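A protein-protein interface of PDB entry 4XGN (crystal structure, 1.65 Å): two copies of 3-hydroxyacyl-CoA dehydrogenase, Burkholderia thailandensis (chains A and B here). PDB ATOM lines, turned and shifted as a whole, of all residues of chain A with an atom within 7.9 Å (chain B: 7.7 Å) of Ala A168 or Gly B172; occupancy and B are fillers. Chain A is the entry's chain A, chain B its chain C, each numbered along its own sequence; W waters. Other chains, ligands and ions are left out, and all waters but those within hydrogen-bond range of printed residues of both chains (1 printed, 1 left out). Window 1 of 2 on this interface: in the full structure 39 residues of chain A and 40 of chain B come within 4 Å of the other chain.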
ATOM      1  N   PHE A 112       5.814  11.556   1.787  1.00  0.00           N
ATOM      2  CA  PHE A 112       4.551  11.576   2.514  1.00  0.00           C
ATOM      3  C   PHE A 112       3.895  12.953   2.396  1.00  0.00           C
ATOM      4  O   PHE A 112       2.730  13.086   2.001  1.00  0.00           O
ATOM      5  CB  PHE A 112       4.769  11.214   3.991  1.00  0.00           C
ATOM      6  CG  PHE A 112       3.481  11.037   4.771  1.00  0.00           C
ATOM      7  CD1 PHE A 112       2.868  12.118   5.391  1.00  0.00           C
ATOM      8  CD2 PHE A 112       2.921   9.795   4.895  1.00  0.00           C
ATOM      9  CE1 PHE A 112       1.680  11.962   6.108  1.00  0.00           C
ATOM     10  CE2 PHE A 112       1.746   9.615   5.635  1.00  0.00           C
ATOM     11  CZ  PHE A 112       1.127  10.700   6.234  1.00  0.00           C
ATOM     12  N   THR A 115       2.486  13.682  -1.158  1.00  0.00           N
ATOM     13  CA  THR A 115       1.241  12.925  -1.438  1.00  0.00           C
ATOM     14  C   THR A 115       0.051  13.573  -0.762  1.00  0.00           C
ATOM     15  O   THR A 115      -1.034  13.739  -1.342  1.00  0.00           O
ATOM     16  CB  THR A 115       1.410  11.477  -0.944  1.00  0.00           C
ATOM     17  OG1 THR A 115       2.533  10.908  -1.617  1.00  0.00           O
ATOM     18  CG2 THR A 115       0.150  10.637  -1.227  1.00  0.00           C
ATOM     19  N   ILE A 116       0.241  13.901   0.509  1.00  0.00           N
ATOM     20  CA  ILE A 116      -0.784  14.584   1.289  1.00  0.00           C
ATOM     21  C   ILE A 116      -1.124  15.950   0.670  1.00  0.00           C
ATOM     22  O   ILE A 116      -2.303  16.336   0.613  1.00  0.00           O
ATOM     23  CB  ILE A 116      -0.376  14.695   2.778  1.00  0.00           C
ATOM     24  CG1 ILE A 116      -0.882  13.482   3.538  1.00  0.00           C
ATOM     25  CG2 ILE A 116      -0.949  15.936   3.453  1.00  0.00           C
ATOM     26  CD1 ILE A 116      -0.351  12.125   3.100  1.00  0.00           C
ATOM     27  N   ASN A 119      -3.032  15.299  -2.828  1.00  0.00           N
ATOM     28  CA  ASN A 119      -4.264  14.547  -2.780  1.00  0.00           C
ATOM     29  C   ASN A 119      -5.276  15.107  -1.821  1.00  0.00           C
ATOM     30  O   ASN A 119      -6.465  15.027  -2.090  1.00  0.00           O
ATOM     31  CB  ASN A 119      -3.961  13.100  -2.390  1.00  0.00           C
ATOM     32  CG  ASN A 119      -3.210  12.322  -3.460  1.00  0.00           C
ATOM     33  OD1 ASN A 119      -2.906  12.835  -4.551  1.00  0.00           O
ATOM     34  ND2 ASN A 119      -2.952  11.058  -3.175  1.00  0.00           N
ATOM     35  N   LEU A 120      -4.816  15.625  -0.683  1.00  0.00           N
ATOM     36  CA  LEU A 120      -5.700  16.030   0.376  1.00  0.00           C
ATOM     37  C   LEU A 120      -5.799  17.543   0.441  1.00  0.00           C
ATOM     38  O   LEU A 120      -6.885  18.089   0.301  1.00  0.00           O
ATOM     39  CB  LEU A 120      -5.259  15.381   1.709  1.00  0.00           C
ATOM     40  CG  LEU A 120      -6.067  15.753   2.954  1.00  0.00           C
ATOM     41  CD1 LEU A 120      -7.569  15.569   2.772  1.00  0.00           C
ATOM     42  CD2 LEU A 120      -5.560  14.991   4.152  1.00  0.00           C
ATOM     43  N   ALA A 155      -7.919   2.413  -0.834  1.00  0.00           N
ATOM     44  CA  ALA A 155      -6.790   2.546   0.082  1.00  0.00           C
ATOM     45  C   ALA A 155      -7.132   3.359   1.352  1.00  0.00           C
ATOM     46  O   ALA A 155      -6.392   3.258   2.336  1.00  0.00           O
ATOM     47  CB  ALA A 155      -5.586   3.190  -0.624  1.00  0.00           C
ATOM     48  N   ALA A 156      -8.209   4.141   1.344  1.00  0.00           N
ATOM     49  CA  ALA A 156      -8.742   4.789   2.537  1.00  0.00           C
ATOM     50  C   ALA A 156      -9.078   3.761   3.626  1.00  0.00           C
ATOM     51  O   ALA A 156      -9.057   4.114   4.804  1.00  0.00           O
ATOM     52  CB  ALA A 156      -9.981   5.644   2.242  1.00  0.00           C
ATOM     53  N   GLY A 159      -5.634  -0.016   3.031  1.00  0.00           N
ATOM     54  CA  GLY A 159      -4.278   0.412   2.615  1.00  0.00           C
ATOM     55  C   GLY A 159      -3.280  -0.745   2.641  1.00  0.00           C
ATOM     56  O   GLY A 159      -3.197  -1.465   3.626  1.00  0.00           O
ATOM     57  N   GLN A 163       1.598   1.816   1.047  1.00  0.00           N
ATOM     58  CA  GLN A 163       0.592   2.841   0.797  1.00  0.00           C
ATOM     59  C   GLN A 163       0.249   3.741   1.976  1.00  0.00           C
ATOM     60  O   GLN A 163      -0.795   4.385   1.978  1.00  0.00           O
ATOM     61  CB  GLN A 163      -0.720   2.218   0.340  1.00  0.00           C
ATOM     62  CG  GLN A 163      -0.706   1.485  -0.944  1.00  0.00           C
ATOM     63  CD  GLN A 163      -2.134   1.248  -1.418  1.00  0.00           C
ATOM     64  OE1 GLN A 163      -2.947   0.737  -0.670  1.00  0.00           O
ATOM     65  NE2 GLN A 163      -2.471   1.664  -2.661  1.00  0.00           N
ATOM     66  N   ALA A 164       1.110   3.825   2.982  1.00  0.00           N
ATOM     67  CA  ALA A 164       0.790   4.684   4.120  1.00  0.00           C
ATOM     68  C   ALA A 164       0.460   6.131   3.728  1.00  0.00           C
ATOM     69  O   ALA A 164      -0.575   6.677   4.149  1.00  0.00           O
ATOM     70  CB  ALA A 164       1.878   4.644   5.141  1.00  0.00           C
ATOM     71  N   ALA A 165       1.274   6.723   2.861  1.00  0.00           N
ATOM     72  CA  ALA A 165       1.015   8.096   2.426  1.00  0.00           C
ATOM     73  C   ALA A 165      -0.277   8.231   1.616  1.00  0.00           C
ATOM     74  O   ALA A 165      -1.105   9.087   1.907  1.00  0.00           O
ATOM     75  CB  ALA A 165       2.157   8.647   1.610  1.00  0.00           C
ATOM     76  N   TYR A 166      -0.440   7.368   0.626  1.00  0.00           N
ATOM     77  CA  TYR A 166      -1.634   7.382  -0.222  1.00  0.00           C
ATOM     78  C   TYR A 166      -2.897   7.110   0.603  1.00  0.00           C
ATOM     79  O   TYR A 166      -3.854   7.854   0.528  1.00  0.00           O
ATOM     80  CB  TYR A 166      -1.474   6.345  -1.305  1.00  0.00           C
ATOM     81  CG  TYR A 166      -2.550   6.374  -2.365  1.00  0.00           C
ATOM     82  CD1 TYR A 166      -2.663   7.438  -3.229  1.00  0.00           C
ATOM     83  CD2 TYR A 166      -3.372   5.298  -2.551  1.00  0.00           C
ATOM     84  CE1 TYR A 166      -3.604   7.446  -4.232  1.00  0.00           C
ATOM     85  CE2 TYR A 166      -4.341   5.297  -3.540  1.00  0.00           C
ATOM     86  CZ  TYR A 166      -4.424   6.364  -4.405  1.00  0.00           C
ATOM     87  OH  TYR A 166      -5.352   6.397  -5.445  1.00  0.00           O
ATOM     88  N   ALA A 167      -2.830   6.099   1.460  1.00  0.00           N
ATOM     89  CA  ALA A 167      -3.963   5.783   2.309  1.00  0.00           C
ATOM     90  C   ALA A 167      -4.307   6.926   3.256  1.00  0.00           C
ATOM     91  O   ALA A 167      -5.470   7.298   3.402  1.00  0.00           O
ATOM     92  CB  ALA A 167      -3.681   4.536   3.113  1.00  0.00           C
ATOM     93  N   ALA A 168      -3.293   7.528   3.872  1.00  0.00           N
ATOM     94  CA  ALA A 168      -3.557   8.708   4.709  1.00  0.00           C
ATOM     95  C   ALA A 168      -4.277   9.807   3.961  1.00  0.00           C
ATOM     96  O   ALA A 168      -5.231  10.359   4.436  1.00  0.00           O
ATOM     97  CB  ALA A 168      -2.278   9.250   5.307  1.00  0.00           C
ATOM     98  N   SER A 169      -3.780  10.125   2.777  1.00  0.00           N
ATOM     99  CA  SER A 169      -4.370  11.146   1.989  1.00  0.00           C
ATOM    100  C   SER A 169      -5.787  10.859   1.576  1.00  0.00           C
ATOM    101  O   SER A 169      -6.628  11.746   1.632  1.00  0.00           O
ATOM    102  CB  SER A 169      -3.489  11.481   0.773  1.00  0.00           C
ATOM    103  OG  SER A 169      -3.620  10.522  -0.278  1.00  0.00           O
ATOM    104  N   LYS A 170      -6.062   9.637   1.175  1.00  0.00           N
ATOM    105  CA  LYS A 170      -7.377   9.289   0.688  1.00  0.00           C
ATOM    106  C   LYS A 170      -8.383   9.077   1.834  1.00  0.00           C
ATOM    107  O   LYS A 170      -9.558   9.382   1.703  1.00  0.00           O
ATOM    108  CB  LYS A 170      -7.268   8.075  -0.223  1.00  0.00           C
ATOM    109  CG  LYS A 170      -6.445   8.315  -1.459  1.00  0.00           C
ATOM    110  CD  LYS A 170      -6.921   9.483  -2.240  1.00  0.00           C
ATOM    111  CE  LYS A 170      -6.435   9.424  -3.666  1.00  0.00           C
ATOM    112  NZ  LYS A 170      -7.197  10.289  -4.560  1.00  0.00           N
ATOM    113  N   ALA A 171      -7.925   8.586   2.974  1.00  0.00           N
ATOM    114  CA  ALA A 171      -8.792   8.549   4.172  1.00  0.00           C
ATOM    115  C   ALA A 171      -9.141   9.951   4.639  1.00  0.00           C
ATOM    116  O   ALA A 171     -10.250  10.198   5.103  1.00  0.00           O
ATOM    117  CB  ALA A 171      -8.067   7.801   5.289  1.00  0.00           C
ATOM    118  N   GLY A 172      -8.192  10.872   4.546  1.00  0.00           N
ATOM    119  CA  GLY A 172      -8.476  12.299   4.802  1.00  0.00           C
ATOM    120  C   GLY A 172      -9.610  12.862   3.930  1.00  0.00           C
ATOM    121  O   GLY A 172     -10.563  13.500   4.407  1.00  0.00           O
ATOM    122  N   VAL A 173      -9.522  12.571   2.638  1.00  0.00           N
ATOM    123  CA  VAL A 173     -10.539  13.008   1.655  1.00  0.00           C
ATOM    124  C   VAL A 173     -11.881  12.380   2.041  1.00  0.00           C
ATOM    125  O   VAL A 173     -12.896  13.087   2.154  1.00  0.00           O
ATOM    126  CB  VAL A 173     -10.134  12.636   0.210  1.00  0.00           C
ATOM    127  CG1 VAL A 173     -11.321  12.831  -0.755  1.00  0.00           C
ATOM    128  CG2 VAL A 173      -8.940  13.448  -0.245  1.00  0.00           C
ATOM    129  N   ALA A 174     -11.872  11.062   2.280  1.00  0.00           N
ATOM    130  CA  ALA A 174     -13.112  10.382   2.688  1.00  0.00           C
ATOM    131  C   ALA A 174     -13.704  11.003   3.953  1.00  0.00           C
ATOM    132  O   ALA A 174     -14.909  11.301   4.019  1.00  0.00           O
ATOM    133  CB  ALA A 174     -12.876   8.897   2.853  1.00  0.00           C
ATOM    134  N   GLY A 175     -12.887  11.141   4.971  1.00  0.00           N
ATOM    135  CA  GLY A 175     -13.361  11.603   6.279  1.00  0.00           C
ATOM    136  C   GLY A 175     -13.837  13.054   6.329  1.00  0.00           C
ATOM    137  O   GLY A 175     -14.664  13.370   7.163  1.00  0.00           O
ATOM    138  N   MET A 176     -13.363  13.914   5.430  1.00  0.00           N
ATOM    139  CA  MET A 176     -13.839  15.288   5.396  1.00  0.00           C
ATOM    140  C   MET A 176     -15.124  15.462   4.624  1.00  0.00           C
ATOM    141  O   MET A 176     -15.728  16.536   4.686  1.00  0.00           O
ATOM    142  CB  MET A 176     -12.763  16.279   4.921  1.00  0.00           C
ATOM    143  CG  MET A 176     -12.482  16.294   3.474  1.00  0.00           C
ATOM    144  SD  MET A 176     -11.049  17.408   3.150  1.00  0.00           S
ATOM    145  CE  MET A 176     -11.015  17.336   1.379  1.00  0.00           C
ATOM    146  N   ASN B 119      -1.008  17.551  12.687  1.00  0.00           N
ATOM    147  CA  ASN B 119      -1.746  16.398  13.159  1.00  0.00           C
ATOM    148  C   ASN B 119      -1.449  15.142  12.367  1.00  0.00           C
ATOM    149  O   ASN B 119      -1.407  14.054  12.972  1.00  0.00           O
ATOM    150  CB  ASN B 119      -3.254  16.632  13.099  1.00  0.00           C
ATOM    151  CG  ASN B 119      -3.732  17.655  14.069  1.00  0.00           C
ATOM    152  OD1 ASN B 119      -2.948  18.208  14.868  1.00  0.00           O
ATOM    153  ND2 ASN B 119      -5.032  17.957  14.024  1.00  0.00           N
ATOM    154  N   LEU B 120      -1.297  15.251  11.045  1.00  0.00           N
ATOM    155  CA  LEU B 120      -1.188  14.068  10.166  1.00  0.00           C
ATOM    156  C   LEU B 120       0.271  13.867   9.754  1.00  0.00           C
ATOM    157  O   LEU B 120       0.860  12.833  10.024  1.00  0.00           O
ATOM    158  CB  LEU B 120      -2.149  14.194   8.985  1.00  0.00           C
ATOM    159  CG  LEU B 120      -2.052  13.048   7.967  1.00  0.00           C
ATOM    160  CD1 LEU B 120      -2.222  11.676   8.581  1.00  0.00           C
ATOM    161  CD2 LEU B 120      -3.133  13.317   6.926  1.00  0.00           C
ATOM    162  N   ILE B 121       0.894  14.870   9.123  1.00  0.00           N
ATOM    163  CA  ILE B 121       2.300  14.731   8.711  1.00  0.00           C
ATOM    164  C   ILE B 121       3.196  14.531   9.970  1.00  0.00           C
ATOM    165  O   ILE B 121       4.119  13.679   9.968  1.00  0.00           O
ATOM    166  CB  ILE B 121       2.785  15.922   7.852  1.00  0.00           C
ATOM    167  CG1 ILE B 121       1.946  16.001   6.573  1.00  0.00           C
ATOM    168  CG2 ILE B 121       4.269  15.781   7.551  1.00  0.00           C
ATOM    169  CD1 ILE B 121       2.111  17.204   5.691  1.00  0.00           C
ATOM    170  N   THR B 123       2.386  13.283  12.921  1.00  0.00           N
ATOM    171  CA  THR B 123       2.214  11.934  13.478  1.00  0.00           C
ATOM    172  C   THR B 123       2.975  10.916  12.624  1.00  0.00           C
ATOM    173  O   THR B 123       3.691  10.092  13.141  1.00  0.00           O
ATOM    174  CB  THR B 123       0.726  11.546  13.621  1.00  0.00           C
ATOM    175  OG1 THR B 123       0.202  12.169  14.804  1.00  0.00           O
ATOM    176  CG2 THR B 123       0.573  10.061  13.817  1.00  0.00           C
ATOM    177  N   PHE B 124       2.901  11.014  11.301  1.00  0.00           N
ATOM    178  CA  PHE B 124       3.625  10.064  10.490  1.00  0.00           C
ATOM    179  C   PHE B 124       5.140  10.223  10.676  1.00  0.00           C
ATOM    180  O   PHE B 124       5.892   9.236  10.648  1.00  0.00           O
ATOM    181  CB  PHE B 124       3.298  10.175   9.000  1.00  0.00           C
ATOM    182  CG  PHE B 124       4.004   9.154   8.192  1.00  0.00           C
ATOM    183  CD1 PHE B 124       3.560   7.866   8.204  1.00  0.00           C
ATOM    184  CD2 PHE B 124       5.137   9.479   7.422  1.00  0.00           C
ATOM    185  CE1 PHE B 124       4.193   6.872   7.489  1.00  0.00           C
ATOM    186  CE2 PHE B 124       5.767   8.482   6.699  1.00  0.00           C
ATOM    187  CZ  PHE B 124       5.297   7.189   6.731  1.00  0.00           C
ATOM    188  N   ALA B 152      -6.438   9.764  16.932  1.00  0.00           N
ATOM    189  CA  ALA B 152      -7.314  10.364  15.933  1.00  0.00           C
ATOM    190  C   ALA B 152      -8.335  11.223  16.687  1.00  0.00           C
ATOM    191  O   ALA B 152      -7.912  12.096  17.455  1.00  0.00           O
ATOM    192  CB  ALA B 152      -7.927   9.300  15.038  1.00  0.00           C
ATOM    193  N   ALA B 156     -12.851  12.092  12.969  1.00  0.00           N
ATOM    194  CA  ALA B 156     -12.550  11.274  11.778  1.00  0.00           C
ATOM    195  C   ALA B 156     -13.801  10.710  11.142  1.00  0.00           C
ATOM    196  O   ALA B 156     -13.819  10.437   9.967  1.00  0.00           O
ATOM    197  CB  ALA B 156     -11.599  10.159  12.087  1.00  0.00           C
ATOM    198  N   TYR B 166      -9.619  19.555  10.763  1.00  0.00           N
ATOM    199  CA  TYR B 166      -9.326  18.657  11.879  1.00  0.00           C
ATOM    200  C   TYR B 166      -9.794  17.255  11.509  1.00  0.00           C
ATOM    201  O   TYR B 166      -9.066  16.290  11.652  1.00  0.00           O
ATOM    202  CB  TYR B 166     -10.046  19.172  13.109  1.00  0.00           C
ATOM    203  CG  TYR B 166      -9.756  18.407  14.364  1.00  0.00           C
ATOM    204  CD1 TYR B 166      -8.509  18.485  14.928  1.00  0.00           C
ATOM    205  CD2 TYR B 166     -10.737  17.647  14.967  1.00  0.00           C
ATOM    206  CE1 TYR B 166      -8.219  17.811  16.114  1.00  0.00           C
ATOM    207  CE2 TYR B 166     -10.469  16.943  16.127  1.00  0.00           C
ATOM    208  CZ  TYR B 166      -9.208  17.057  16.709  1.00  0.00           C
ATOM    209  OH  TYR B 166      -8.941  16.374  17.881  1.00  0.00           O
ATOM    210  N   ALA B 167     -11.009  17.170  10.988  1.00  0.00           N
ATOM    211  CA  ALA B 167     -11.517  15.890  10.550  1.00  0.00           C
ATOM    212  C   ALA B 167     -10.660  15.221   9.488  1.00  0.00           C
ATOM    213  O   ALA B 167     -10.440  14.023   9.550  1.00  0.00           O
ATOM    214  CB  ALA B 167     -12.952  16.019  10.055  1.00  0.00           C
ATOM    215  N   ALA B 168     -10.260  15.973   8.459  1.00  0.00           N
ATOM    216  CA  ALA B 168      -9.397  15.435   7.434  1.00  0.00           C
ATOM    217  C   ALA B 168      -8.143  14.859   8.070  1.00  0.00           C
ATOM    218  O   ALA B 168      -7.692  13.765   7.751  1.00  0.00           O
ATOM    219  CB  ALA B 168      -8.997  16.544   6.436  1.00  0.00           C
ATOM    220  N   SER B 169      -7.551  15.650   8.942  1.00  0.00           N
ATOM    221  CA  SER B 169      -6.300  15.228   9.542  1.00  0.00           C
ATOM    222  C   SER B 169      -6.438  13.948  10.376  1.00  0.00           C
ATOM    223  O   SER B 169      -5.563  13.071  10.371  1.00  0.00           O
ATOM    224  CB  SER B 169      -5.680  16.375  10.371  1.00  0.00           C
ATOM    225  OG  SER B 169      -6.263  16.551  11.667  1.00  0.00           O
ATOM    226  N   LYS B 170      -7.515  13.870  11.132  1.00  0.00           N
ATOM    227  CA  LYS B 170      -7.722  12.736  12.040  1.00  0.00           C
ATOM    228  C   LYS B 170      -8.216  11.487  11.320  1.00  0.00           C
ATOM    229  O   LYS B 170      -7.899  10.346  11.702  1.00  0.00           O
ATOM    230  CB  LYS B 170      -8.629  13.159  13.173  1.00  0.00           C
ATOM    231  CG  LYS B 170      -8.086  14.296  14.025  1.00  0.00           C
ATOM    232  CD  LYS B 170      -6.758  13.938  14.627  1.00  0.00           C
ATOM    233  CE  LYS B 170      -6.412  14.850  15.790  1.00  0.00           C
ATOM    234  NZ  LYS B 170      -5.380  14.199  16.592  1.00  0.00           N
ATOM    235  N   ALA B 171      -9.003  11.678  10.253  1.00  0.00           N
ATOM    236  CA  ALA B 171      -9.359  10.573   9.392  1.00  0.00           C
ATOM    237  C   ALA B 171      -8.132  10.013   8.705  1.00  0.00           C
ATOM    238  O   ALA B 171      -8.028   8.812   8.474  1.00  0.00           O
ATOM    239  CB  ALA B 171     -10.385  11.016   8.366  1.00  0.00           C
ATOM    240  N   GLY B 172      -7.190  10.895   8.345  1.00  0.00           N
ATOM    241  CA  GLY B 172      -5.915  10.432   7.784  1.00  0.00           C
ATOM    242  C   GLY B 172      -5.127   9.583   8.760  1.00  0.00           C
ATOM    243  O   GLY B 172      -4.665   8.490   8.376  1.00  0.00           O
ATOM    244  N   VAL B 173      -5.076  10.013  10.028  1.00  0.00           N
ATOM    245  CA  VAL B 173      -4.384   9.244  11.091  1.00  0.00           C
ATOM    246  C   VAL B 173      -5.077   7.863  11.241  1.00  0.00           C
ATOM    247  O   VAL B 173      -4.406   6.812  11.245  1.00  0.00           O
ATOM    248  CB  VAL B 173      -4.400   9.971  12.427  1.00  0.00           C
ATOM    249  CG1 VAL B 173      -3.884   9.064  13.553  1.00  0.00           C
ATOM    250  CG2 VAL B 173      -3.494  11.195  12.319  1.00  0.00           C
ATOM    251  N   ALA B 174      -6.407   7.878  11.282  1.00  0.00           N
ATOM    252  CA  ALA B 174      -7.154   6.648  11.463  1.00  0.00           C
ATOM    253  C   ALA B 174      -6.907   5.723  10.262  1.00  0.00           C
ATOM    254  O   ALA B 174      -6.671   4.514  10.434  1.00  0.00           O
ATOM    255  CB  ALA B 174      -8.642   6.950  11.633  1.00  0.00           C
ATOM    256  N   GLY B 175      -7.028   6.255   9.036  1.00  0.00           N
ATOM    257  CA  GLY B 175      -6.917   5.420   7.846  1.00  0.00           C
ATOM    258  C   GLY B 175      -5.534   4.842   7.568  1.00  0.00           C
ATOM    259  O   GLY B 175      -5.398   3.808   6.923  1.00  0.00           O
ATOM    260  N   MET B 176      -4.479   5.472   8.090  1.00  0.00           N
ATOM    261  CA  MET B 176      -3.171   4.920   7.841  1.00  0.00           C
ATOM    262  C   MET B 176      -2.774   3.840   8.844  1.00  0.00           C
ATOM    263  O   MET B 176      -1.741   3.216   8.671  1.00  0.00           O
ATOM    264  CB  MET B 176      -2.123   6.028   7.705  1.00  0.00           C
ATOM    265  CG  MET B 176      -1.790   6.763   8.965  1.00  0.00           C
ATOM    266  SD  MET B 176      -0.526   8.021   8.667  1.00  0.00           S
ATOM    267  CE  MET B 176      -0.265   8.522  10.356  1.00  0.00           C
ATOM    268  N   THR B 177      -3.591   3.603   9.872  1.00  0.00           N
ATOM    269  CA  THR B 177      -3.292   2.581  10.878  1.00  0.00           C
ATOM    270  C   THR B 177      -3.034   1.204  10.247  1.00  0.00           C
ATOM    271  O   THR B 177      -2.014   0.542  10.522  1.00  0.00           O
ATOM    272  CB  THR B 177      -4.419   2.494  11.929  1.00  0.00           C
ATOM    273  OG1 THR B 177      -4.796   3.813  12.351  1.00  0.00           O
ATOM    274  CG2 THR B 177      -3.944   1.724  13.119  1.00  0.00           C
ATOM    275  N   PRO B 179      -2.342   0.233   6.856  1.00  0.00           N
ATOM    276  CA  PRO B 179      -1.163   0.027   6.059  1.00  0.00           C
ATOM    277  C   PRO B 179       0.145   0.098   6.851  1.00  0.00           C
ATOM    278  O   PRO B 179       1.074  -0.654   6.546  1.00  0.00           O
ATOM    279  CB  PRO B 179      -1.249   1.145   4.980  1.00  0.00           C
ATOM    280  CG  PRO B 179      -2.178   2.140   5.567  1.00  0.00           C
ATOM    281  CD  PRO B 179      -3.186   1.269   6.290  1.00  0.00           C
ATOM    282  N   ILE B 180       0.209   0.959   7.867  1.00  0.00           N
ATOM    283  CA  ILE B 180       1.424   0.999   8.687  1.00  0.00           C
ATOM    284  C   ILE B 180       1.569  -0.302   9.517  1.00  0.00           C
ATOM    285  O   ILE B 180       2.691  -0.837   9.621  1.00  0.00           O
ATOM    286  CB  ILE B 180       1.470   2.250   9.577  1.00  0.00           C
ATOM    287  CG1 ILE B 180       1.476   3.494   8.686  1.00  0.00           C
ATOM    288  CG2 ILE B 180       2.734   2.227  10.435  1.00  0.00           C
ATOM    289  CD1 ILE B 180       1.331   4.801   9.448  1.00  0.00           C
ATOM    290  N   THR B 193      -4.715   2.963  16.856  1.00  0.00           N
ATOM    291  CA  THR B 193      -5.205   4.317  16.957  1.00  0.00           C
ATOM    292  C   THR B 193      -6.364   4.398  17.931  1.00  0.00           C
ATOM    293  O   THR B 193      -7.229   3.535  17.943  1.00  0.00           O
ATOM    294  CB  THR B 193      -5.637   4.830  15.597  1.00  0.00           C
ATOM    295  OG1 THR B 193      -4.459   4.910  14.785  1.00  0.00           O
ATOM    296  CG2 THR B 193      -6.259   6.213  15.737  1.00  0.00           C
HETATM  297  O   HOH W   1     -15.785  13.182   9.692  1.00  0.00           O
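Hydrophobic or aromatic side chains of chain A that line the printed part of chain B: Phe A112, Ile A116, Ala A164, Ala A167, Ala A168, Ala A171 and Met A176.
Of the 22 printed residues of chain B, 10 touch a printed residue of chain A.
Hydrophobic or aromatic side chains of chain B that line the printed part of chain A: Ile B121, Phe B124, Ala B168, Ala B171, Met B176, Pro B179 and Ile B180.
Among the printed residues, 19 pairs touch across the chains.
Among the printed residues, pairs that only touch across the chains: Ala A171 with Ala B171, Phe A112 with Phe B124, Gly A172 with Ala B168, Ala A168 with Gly B172, Gly A159 with Pro B179, Ala A171 with Gly B175, Gly A175 with Ala B171, Ala A167 with Pro B179, Ala A164 with Ile B180, Phe A112 with Ile B121, Gly A175 with Ala B156, Gly A172 with Gly B172, Ala A164 with Met B176, Ala A156 with Gly B175, Met A176 with Ala B168, Phe A112 with Met B176, Ala A164 with Phe B124, Ala A168 with Met B176 and Ile A116 with Ile B121.
Gly B172 touches just these residues of chain A: Ala A168 (3.4 Å) and Gly A172 (3.9 Å).
Of chain B, only Pro B179 (3.7 Å) comes within 4 Å of Ala A167.
Ala B171 touches just these residues of chain A: Ala A171 (3.3 Å) and Gly A175 (3.7 Å).
Of the printed residues of chain A, Ala B168 touches Gly A172 and Met A176.
Of the printed residues of chain B, Met A176 touches Ala B168.
Of the printed residues of chain B, Phe A112 touches Ile B121, Phe B124 and Met B176.
Of the printed residues of chain A, Phe B124 touches Phe A112 (3.4 Å) and Ala A164 (3.98 Å).
Of the printed residues of chain A, Pro B179 touches Gly A159 (3.5 Å) and Ala A167 (3.7 Å).
Tyr B166 touches none of the printed residues of chain A.
The nearest printed residue of chain B that does not touch Ala A168 is Leu B120 (4.1 Å).
The nearest printed residue of chain B that does not touch Gly A172 is Ala B171 (4.2 Å).
Ala A156 touches Gly B175, and with the chains exchanged Gly A175 touches Ala B156.
Ala A168 touches Gly B172, and with the chains exchanged Gly A172 touches Ala B168.
Ala A171 touches Gly B175, and with the chains exchanged Gly A175 touches Ala B171.
Gly A172 touches its own counterpart, Gly B172.
Positions printed for both chains: 119, 120, 156, 166, 167, 168, 169, 170, 171, 172, 173, 174, 175 and 176.
Water W1 bridges the backbone carbonyl oxygen (O) of Gly A175 (2.8 Å) and the backbone carbonyl oxygen (O) of Ala B156 (3.4 Å).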
